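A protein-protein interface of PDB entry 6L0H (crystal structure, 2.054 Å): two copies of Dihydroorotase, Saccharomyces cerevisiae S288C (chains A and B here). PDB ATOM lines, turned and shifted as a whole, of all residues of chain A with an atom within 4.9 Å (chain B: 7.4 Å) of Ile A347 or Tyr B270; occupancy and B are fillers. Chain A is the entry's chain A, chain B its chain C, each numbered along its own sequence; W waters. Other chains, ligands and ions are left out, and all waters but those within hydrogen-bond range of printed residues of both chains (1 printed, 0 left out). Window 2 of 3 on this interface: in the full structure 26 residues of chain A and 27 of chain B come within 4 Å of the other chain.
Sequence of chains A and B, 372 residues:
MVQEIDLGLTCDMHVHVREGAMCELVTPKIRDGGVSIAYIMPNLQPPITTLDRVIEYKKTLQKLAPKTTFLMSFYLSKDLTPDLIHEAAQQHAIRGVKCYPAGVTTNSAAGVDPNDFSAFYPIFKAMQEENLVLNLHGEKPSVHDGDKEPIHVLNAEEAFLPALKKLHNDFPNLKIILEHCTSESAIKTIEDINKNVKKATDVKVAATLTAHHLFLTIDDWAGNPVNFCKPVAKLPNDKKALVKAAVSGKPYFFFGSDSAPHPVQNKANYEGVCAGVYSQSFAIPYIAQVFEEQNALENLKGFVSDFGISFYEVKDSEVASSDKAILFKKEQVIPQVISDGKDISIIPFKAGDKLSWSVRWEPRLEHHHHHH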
ATOM      1  N   ASN A 224       4.605 -25.602 -17.678  1.00  0.00           N
ATOM      2  CA  ASN A 224       5.879 -24.951 -18.011  1.00  0.00           C
ATOM      3  C   ASN A 224       6.823 -25.099 -16.831  1.00  0.00           C
ATOM      4  O   ASN A 224       6.953 -24.185 -16.002  1.00  0.00           O
ATOM      5  CB  ASN A 224       5.698 -23.480 -18.377  1.00  0.00           C
ATOM      6  CG  ASN A 224       4.751 -23.285 -19.538  1.00  0.00           C
ATOM      7  OD1 ASN A 224       4.909 -23.901 -20.594  1.00  0.00           O
ATOM      8  ND2 ASN A 224       3.756 -22.420 -19.353  1.00  0.00           N
ATOM      9  N   PRO A 225       7.517 -26.222 -16.742  1.00  0.00           N
ATOM     10  CA  PRO A 225       8.492 -26.396 -15.659  1.00  0.00           C
ATOM     11  C   PRO A 225       9.485 -25.258 -15.540  1.00  0.00           C
ATOM     12  O   PRO A 225       9.993 -25.039 -14.437  1.00  0.00           O
ATOM     13  CB  PRO A 225       9.178 -27.718 -16.026  1.00  0.00           C
ATOM     14  CG  PRO A 225       8.109 -28.481 -16.742  1.00  0.00           C
ATOM     15  CD  PRO A 225       7.327 -27.463 -17.521  1.00  0.00           C
ATOM     16  N   VAL A 226       9.774 -24.524 -16.622  1.00  0.00           N
ATOM     17  CA  VAL A 226      10.706 -23.396 -16.540  1.00  0.00           C
ATOM     18  C   VAL A 226      10.204 -22.335 -15.560  1.00  0.00           C
ATOM     19  O   VAL A 226      10.999 -21.586 -14.976  1.00  0.00           O
ATOM     20  CB  VAL A 226      10.963 -22.793 -17.946  1.00  0.00           C
ATOM     21  CG1 VAL A 226       9.783 -21.930 -18.423  1.00  0.00           C
ATOM     22  CG2 VAL A 226      12.234 -21.969 -17.956  1.00  0.00           C
ATOM     23  N   VAL A 264      19.397 -26.623 -18.185  1.00  0.00           N
ATOM     24  CA  VAL A 264      18.112 -26.837 -18.854  1.00  0.00           C
ATOM     25  C   VAL A 264      17.670 -28.300 -18.777  1.00  0.00           C
ATOM     26  O   VAL A 264      16.470 -28.588 -18.666  1.00  0.00           O
ATOM     27  CB  VAL A 264      18.180 -26.337 -20.312  1.00  0.00           C
ATOM     28  CG1 VAL A 264      19.154 -27.180 -21.139  1.00  0.00           C
ATOM     29  CG2 VAL A 264      16.808 -26.332 -20.932  1.00  0.00           C
ATOM     30  N   LYS A 267      15.502 -29.045 -15.954  1.00  0.00           N
ATOM     31  CA  LYS A 267      14.126 -28.576 -16.016  1.00  0.00           C
ATOM     32  C   LYS A 267      13.273 -29.400 -16.971  1.00  0.00           C
ATOM     33  O   LYS A 267      12.056 -29.490 -16.782  1.00  0.00           O
ATOM     34  CB  LYS A 267      14.089 -27.101 -16.431  1.00  0.00           C
ATOM     35  CG  LYS A 267      14.925 -26.137 -15.550  1.00  0.00           C
ATOM     36  CD  LYS A 267      14.403 -26.047 -14.111  1.00  0.00           C
ATOM     37  CE  LYS A 267      12.997 -25.459 -14.083  1.00  0.00           C
ATOM     38  NZ  LYS A 267      12.518 -25.011 -12.716  1.00  0.00           N
ATOM     39  N   ALA A 268      13.872 -30.003 -17.996  1.00  0.00           N
ATOM     40  CA  ALA A 268      13.107 -30.733 -19.011  1.00  0.00           C
ATOM     41  C   ALA A 268      13.095 -32.227 -18.681  1.00  0.00           C
ATOM     42  O   ALA A 268      13.648 -33.063 -19.391  1.00  0.00           O
ATOM     43  CB  ALA A 268      13.680 -30.460 -20.393  1.00  0.00           C
ATOM     44  N   TYR A 278      15.520 -18.708 -12.951  1.00  0.00           N
ATOM     45  CA  TYR A 278      16.799 -17.999 -13.022  1.00  0.00           C
ATOM     46  C   TYR A 278      16.565 -16.548 -13.427  1.00  0.00           C
ATOM     47  O   TYR A 278      16.160 -16.273 -14.562  1.00  0.00           O
ATOM     48  CB  TYR A 278      17.775 -18.665 -13.990  1.00  0.00           C
ATOM     49  CG  TYR A 278      19.037 -17.852 -14.102  1.00  0.00           C
ATOM     50  CD1 TYR A 278      19.934 -17.786 -13.041  1.00  0.00           C
ATOM     51  CD2 TYR A 278      19.299 -17.088 -15.226  1.00  0.00           C
ATOM     52  CE1 TYR A 278      21.076 -17.024 -13.121  1.00  0.00           C
ATOM     53  CE2 TYR A 278      20.431 -16.324 -15.322  1.00  0.00           C
ATOM     54  CZ  TYR A 278      21.330 -16.292 -14.269  1.00  0.00           C
ATOM     55  OH  TYR A 278      22.469 -15.505 -14.350  1.00  0.00           O
ATOM     56  N   GLN A 336      17.403 -16.219 -25.252  1.00  0.00           N
ATOM     57  CA  GLN A 336      16.707 -17.493 -25.091  1.00  0.00           C
ATOM     58  C   GLN A 336      17.399 -18.390 -24.076  1.00  0.00           C
ATOM     59  O   GLN A 336      16.759 -19.250 -23.465  1.00  0.00           O
ATOM     60  CB  GLN A 336      16.646 -18.245 -26.428  1.00  0.00           C
ATOM     61  CG  GLN A 336      15.910 -17.513 -27.549  1.00  0.00           C
ATOM     62  CD  GLN A 336      14.457 -17.257 -27.207  1.00  0.00           C
ATOM     63  OE1 GLN A 336      14.034 -16.115 -27.015  1.00  0.00           O
ATOM     64  NE2 GLN A 336      13.689 -18.324 -27.106  1.00  0.00           N
ATOM     65  N   VAL A 337      18.706 -18.225 -23.918  1.00  0.00           N
ATOM     66  CA  VAL A 337      19.501 -19.091 -23.076  1.00  0.00           C
ATOM     67  C   VAL A 337      20.654 -18.275 -22.522  1.00  0.00           C
ATOM     68  O   VAL A 337      21.108 -17.305 -23.133  1.00  0.00           O
ATOM     69  CB  VAL A 337      20.004 -20.317 -23.860  1.00  0.00           C
ATOM     70  CG1 VAL A 337      21.049 -19.884 -24.868  1.00  0.00           C
ATOM     71  CG2 VAL A 337      20.586 -21.318 -22.925  1.00  0.00           C
ATOM     72  N   SER A 345      23.653 -24.678 -20.115  1.00  0.00           N
ATOM     73  CA  SER A 345      22.687 -23.724 -20.637  1.00  0.00           C
ATOM     74  C   SER A 345      21.591 -23.531 -19.605  1.00  0.00           C
ATOM     75  O   SER A 345      21.048 -24.511 -19.094  1.00  0.00           O
ATOM     76  CB  SER A 345      22.081 -24.231 -21.943  1.00  0.00           C
ATOM     77  OG  SER A 345      23.080 -24.337 -22.925  1.00  0.00           O
ATOM     78  N   ILE A 346      21.244 -22.279 -19.317  1.00  0.00           N
ATOM     79  CA  ILE A 346      20.144 -21.970 -18.412  1.00  0.00           C
ATOM     80  C   ILE A 346      19.105 -21.186 -19.185  1.00  0.00           C
ATOM     81  O   ILE A 346      19.454 -20.257 -19.917  1.00  0.00           O
ATOM     82  CB  ILE A 346      20.599 -21.138 -17.192  1.00  0.00           C
ATOM     83  CG1 ILE A 346      21.861 -21.710 -16.531  1.00  0.00           C
ATOM     84  CG2 ILE A 346      19.446 -20.997 -16.205  1.00  0.00           C
ATOM     85  CD1 ILE A 346      22.647 -20.599 -15.774  1.00  0.00           C
ATOM     86  N   ILE A 347      17.828 -21.487 -18.974  1.00  0.00           N
ATOM     87  CA  ILE A 347      16.748 -20.696 -19.554  1.00  0.00           C
ATOM     88  C   ILE A 347      16.438 -19.571 -18.576  1.00  0.00           C
ATOM     89  O   ILE A 347      16.051 -19.857 -17.432  1.00  0.00           O
ATOM     90  CB  ILE A 347      15.481 -21.510 -19.837  1.00  0.00           C
ATOM     91  CG1 ILE A 347      15.801 -22.851 -20.518  1.00  0.00           C
ATOM     92  CG2 ILE A 347      14.526 -20.636 -20.657  1.00  0.00           C
ATOM     93  CD1 ILE A 347      16.518 -22.721 -21.853  1.00  0.00           C
ATOM     94  N   PRO A 348      16.621 -18.312 -18.961  1.00  0.00           N
ATOM     95  CA  PRO A 348      16.348 -17.202 -18.048  1.00  0.00           C
ATOM     96  C   PRO A 348      14.865 -16.875 -18.007  1.00  0.00           C
ATOM     97  O   PRO A 348      14.115 -17.123 -18.953  1.00  0.00           O
ATOM     98  CB  PRO A 348      17.127 -16.046 -18.671  1.00  0.00           C
ATOM     99  CG  PRO A 348      16.999 -16.343 -20.170  1.00  0.00           C
ATOM    100  CD  PRO A 348      17.090 -17.840 -20.281  1.00  0.00           C
ATOM    101  N   PHE A 349      14.477 -16.265 -16.892  1.00  0.00           N
ATOM    102  CA  PHE A 349      13.103 -15.835 -16.680  1.00  0.00           C
ATOM    103  C   PHE A 349      12.655 -14.906 -17.800  1.00  0.00           C
ATOM    104  O   PHE A 349      13.388 -14.013 -18.231  1.00  0.00           O
ATOM    105  CB  PHE A 349      13.000 -15.129 -15.320  1.00  0.00           C
ATOM    106  CG  PHE A 349      11.617 -14.628 -14.991  1.00  0.00           C
ATOM    107  CD1 PHE A 349      10.529 -15.490 -15.024  1.00  0.00           C
ATOM    108  CD2 PHE A 349      11.411 -13.297 -14.626  1.00  0.00           C
ATOM    109  CE1 PHE A 349       9.256 -15.031 -14.738  1.00  0.00           C
ATOM    110  CE2 PHE A 349      10.130 -12.830 -14.316  1.00  0.00           C
ATOM    111  CZ  PHE A 349       9.065 -13.689 -14.382  1.00  0.00           C
ATOM    112  N   ALA A 351      12.385 -15.416 -20.894  1.00  0.00           N
ATOM    113  CA  ALA A 351      13.196 -15.549 -22.102  1.00  0.00           C
ATOM    114  C   ALA A 351      12.414 -15.082 -23.325  1.00  0.00           C
ATOM    115  O   ALA A 351      11.265 -15.472 -23.521  1.00  0.00           O
ATOM    116  CB  ALA A 351      13.641 -17.002 -22.289  1.00  0.00           C
ATOM    117  N   LYS B 267       6.713 -35.144 -22.817  1.00  0.00           N
ATOM    118  CA  LYS B 267       6.560 -34.785 -21.417  1.00  0.00           C
ATOM    119  C   LYS B 267       7.797 -34.118 -20.838  1.00  0.00           C
ATOM    120  O   LYS B 267       7.678 -33.306 -19.918  1.00  0.00           O
ATOM    121  CB  LYS B 267       6.215 -36.023 -20.595  1.00  0.00           C
ATOM    122  CG  LYS B 267       4.876 -36.618 -20.945  1.00  0.00           C
ATOM    123  CD  LYS B 267       3.775 -35.621 -20.640  1.00  0.00           C
ATOM    124  CE  LYS B 267       2.529 -36.314 -20.206  1.00  0.00           C
ATOM    125  NZ  LYS B 267       1.684 -35.426 -19.392  1.00  0.00           N
ATOM    126  N   ALA B 268       8.975 -34.413 -21.369  1.00  0.00           N
ATOM    127  CA  ALA B 268      10.224 -33.907 -20.806  1.00  0.00           C
ATOM    128  C   ALA B 268      10.621 -32.628 -21.538  1.00  0.00           C
ATOM    129  O   ALA B 268      11.592 -32.576 -22.294  1.00  0.00           O
ATOM    130  CB  ALA B 268      11.310 -34.975 -20.895  1.00  0.00           C
ATOM    131  N   ASN B 269       9.790 -31.606 -21.339  1.00  0.00           N
ATOM    132  CA  ASN B 269       9.960 -30.281 -21.913  1.00  0.00           C
ATOM    133  C   ASN B 269      10.117 -29.253 -20.800  1.00  0.00           C
ATOM    134  O   ASN B 269       9.480 -29.369 -19.752  1.00  0.00           O
ATOM    135  CB  ASN B 269       8.748 -29.870 -22.753  1.00  0.00           C
ATOM    136  CG  ASN B 269       8.607 -30.677 -24.019  1.00  0.00           C
ATOM    137  OD1 ASN B 269       9.169 -31.760 -24.123  1.00  0.00           O
ATOM    138  ND2 ASN B 269       7.839 -30.158 -24.994  1.00  0.00           N
ATOM    139  N   TYR B 270      10.904 -28.198 -21.048  1.00  0.00           N
ATOM    140  CA  TYR B 270      10.915 -27.113 -20.070  1.00  0.00           C
ATOM    141  C   TYR B 270       9.727 -26.174 -20.246  1.00  0.00           C
ATOM    142  O   TYR B 270       9.407 -25.419 -19.319  1.00  0.00           O
ATOM    143  CB  TYR B 270      12.240 -26.335 -20.101  1.00  0.00           C
ATOM    144  CG  TYR B 270      12.580 -25.511 -21.338  1.00  0.00           C
ATOM    145  CD1 TYR B 270      13.582 -25.922 -22.210  1.00  0.00           C
ATOM    146  CD2 TYR B 270      11.949 -24.301 -21.600  1.00  0.00           C
ATOM    147  CE1 TYR B 270      13.928 -25.174 -23.309  1.00  0.00           C
ATOM    148  CE2 TYR B 270      12.291 -23.539 -22.713  1.00  0.00           C
ATOM    149  CZ  TYR B 270      13.281 -23.989 -23.560  1.00  0.00           C
ATOM    150  OH  TYR B 270      13.631 -23.242 -24.659  1.00  0.00           O
ATOM    151  N   GLU B 271       9.049 -26.230 -21.392  1.00  0.00           N
ATOM    152  CA  GLU B 271       7.791 -25.526 -21.589  1.00  0.00           C
ATOM    153  C   GLU B 271       6.945 -26.305 -22.589  1.00  0.00           C
ATOM    154  O   GLU B 271       7.461 -27.084 -23.395  1.00  0.00           O
ATOM    155  CB  GLU B 271       8.018 -24.091 -22.066  1.00  0.00           C
ATOM    156  CG  GLU B 271       8.697 -24.003 -23.423  1.00  0.00           C
ATOM    157  CD  GLU B 271       9.120 -22.586 -23.764  1.00  0.00           C
ATOM    158  OE1 GLU B 271       8.754 -21.649 -23.010  1.00  0.00           O
ATOM    159  OE2 GLU B 271       9.815 -22.409 -24.786  1.00  0.00           O
ATOM    160  N   GLY B 272       5.637 -26.089 -22.526  1.00  0.00           N
ATOM    161  CA  GLY B 272       4.736 -26.766 -23.436  1.00  0.00           C
ATOM    162  C   GLY B 272       4.626 -28.257 -23.200  1.00  0.00           C
ATOM    163  O   GLY B 272       4.447 -29.010 -24.151  1.00  0.00           O
ATOM    164  N   VAL B 273       4.733 -28.703 -21.946  1.00  0.00           N
ATOM    165  CA  VAL B 273       4.490 -30.103 -21.619  1.00  0.00           C
ATOM    166  C   VAL B 273       3.099 -30.500 -22.098  1.00  0.00           C
ATOM    167  O   VAL B 273       2.102 -29.850 -21.758  1.00  0.00           O
ATOM    168  CB  VAL B 273       4.609 -30.326 -20.101  1.00  0.00           C
ATOM    169  CG1 VAL B 273       4.001 -31.689 -19.709  1.00  0.00           C
ATOM    170  CG2 VAL B 273       6.063 -30.219 -19.622  1.00  0.00           C
HETATM  171  O   HOH W   1      14.394 -20.100 -24.432  1.00  0.00           O
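The backbone carbonyl oxygen (O) of Pro A225 sits close to the side-chain amino group (NZ) of Lys A267 (3.1 Å).
The backbone NH (N) of Val A264 is in hydrogen-bond range of the backbone carbonyl oxygen (O) of Ser A345 (2.8 Å).
The side-chain amide nitrogen (ND2) of Asn B269 lies close to the backbone carbonyl oxygen (O) of Glu B271.
Water W1 bridges the backbone carbonyl oxygen (O) of Gln A336 (2.7 Å) and the side-chain hydroxyl (OH) of Tyr B270 (3.2 Å).
Ala B268 touches its own counterpart, Ala A268.
Of the 13 pairs that touch across the chains among the printed residues, 1 has its exchanged pair printed and touching as well.
OD1 of Asn A224 lies within hydrogen-bond range of N of Gly B272 (3.0 Å).
O of Tyr B270 sits at hydrogen-bond distance from N of Val A226, at 2.9 Å.
The backbone nitrogen (N) of Pro A225 sits close to the backbone carbonyl oxygen (O) of Tyr B270 (3.3 Å).
Among the printed residues, pairs that only touch across the chains: Ala A268 with Ala B268 (3.4 Å), Pro A225 with Asn B269 (3.4 Å), Asn A224 with Glu B271 (3.4 Å), Val A264 with Tyr B270 (3.5 Å), Asn A224 with Tyr B270 (3.6 Å), Ala A268 with Tyr B270 (3.6 Å), Pro A225 with Val B273 (3.7 Å), Ala A268 with Asn B269 (3.8 Å), Ile A347 with Tyr B270 (3.9 Å) and Lys A267 with Asn B269 (3.9 Å).
Ile A347 touches just one residue of chain B: Tyr B270 (3.9 Å).
Of chain A, only Asn A224 (3.6 Å), Pro A225 (3.3 Å), Val A226 (2.9 Å), Val A264 (3.5 Å), Ala A268 (3.6 Å) and Ile A347 (3.9 Å) come within 4 Å of Tyr B270.
Printed residues of chain A within 4 Å of Glu B271: Asn A224 (3.4 Å).
Of the printed residues of chain A, Ala B268 touches Ala A268 (3.4 Å).
Of the printed residues of chain B, Lys A267 touches Asn B269.
Of the printed residues of chain A, Asn B269 touches Pro A225 (3.4 Å), Lys A267 (3.9 Å) and Ala A268 (3.8 Å).
Ser A345 touches none of the printed residues of chain B.
Phe A349 touches none of the printed residues of chain B.
The nearest residue of chain A that does not touch Tyr B270 is Lys A267 (4.2 Å).
The nearest printed residue of chain A that does not touch Asn B269 is Val A226 (5.8 Å).
Of the 7 printed residues of chain B, 6 touch a printed residue of chain A.
Hydrophobic or aromatic side chains of chain B within 4 Å of the printed part of chain A: Ala B268, Tyr B270 and Val B273.
Among the printed residues, 13 pairs touch across the chains.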
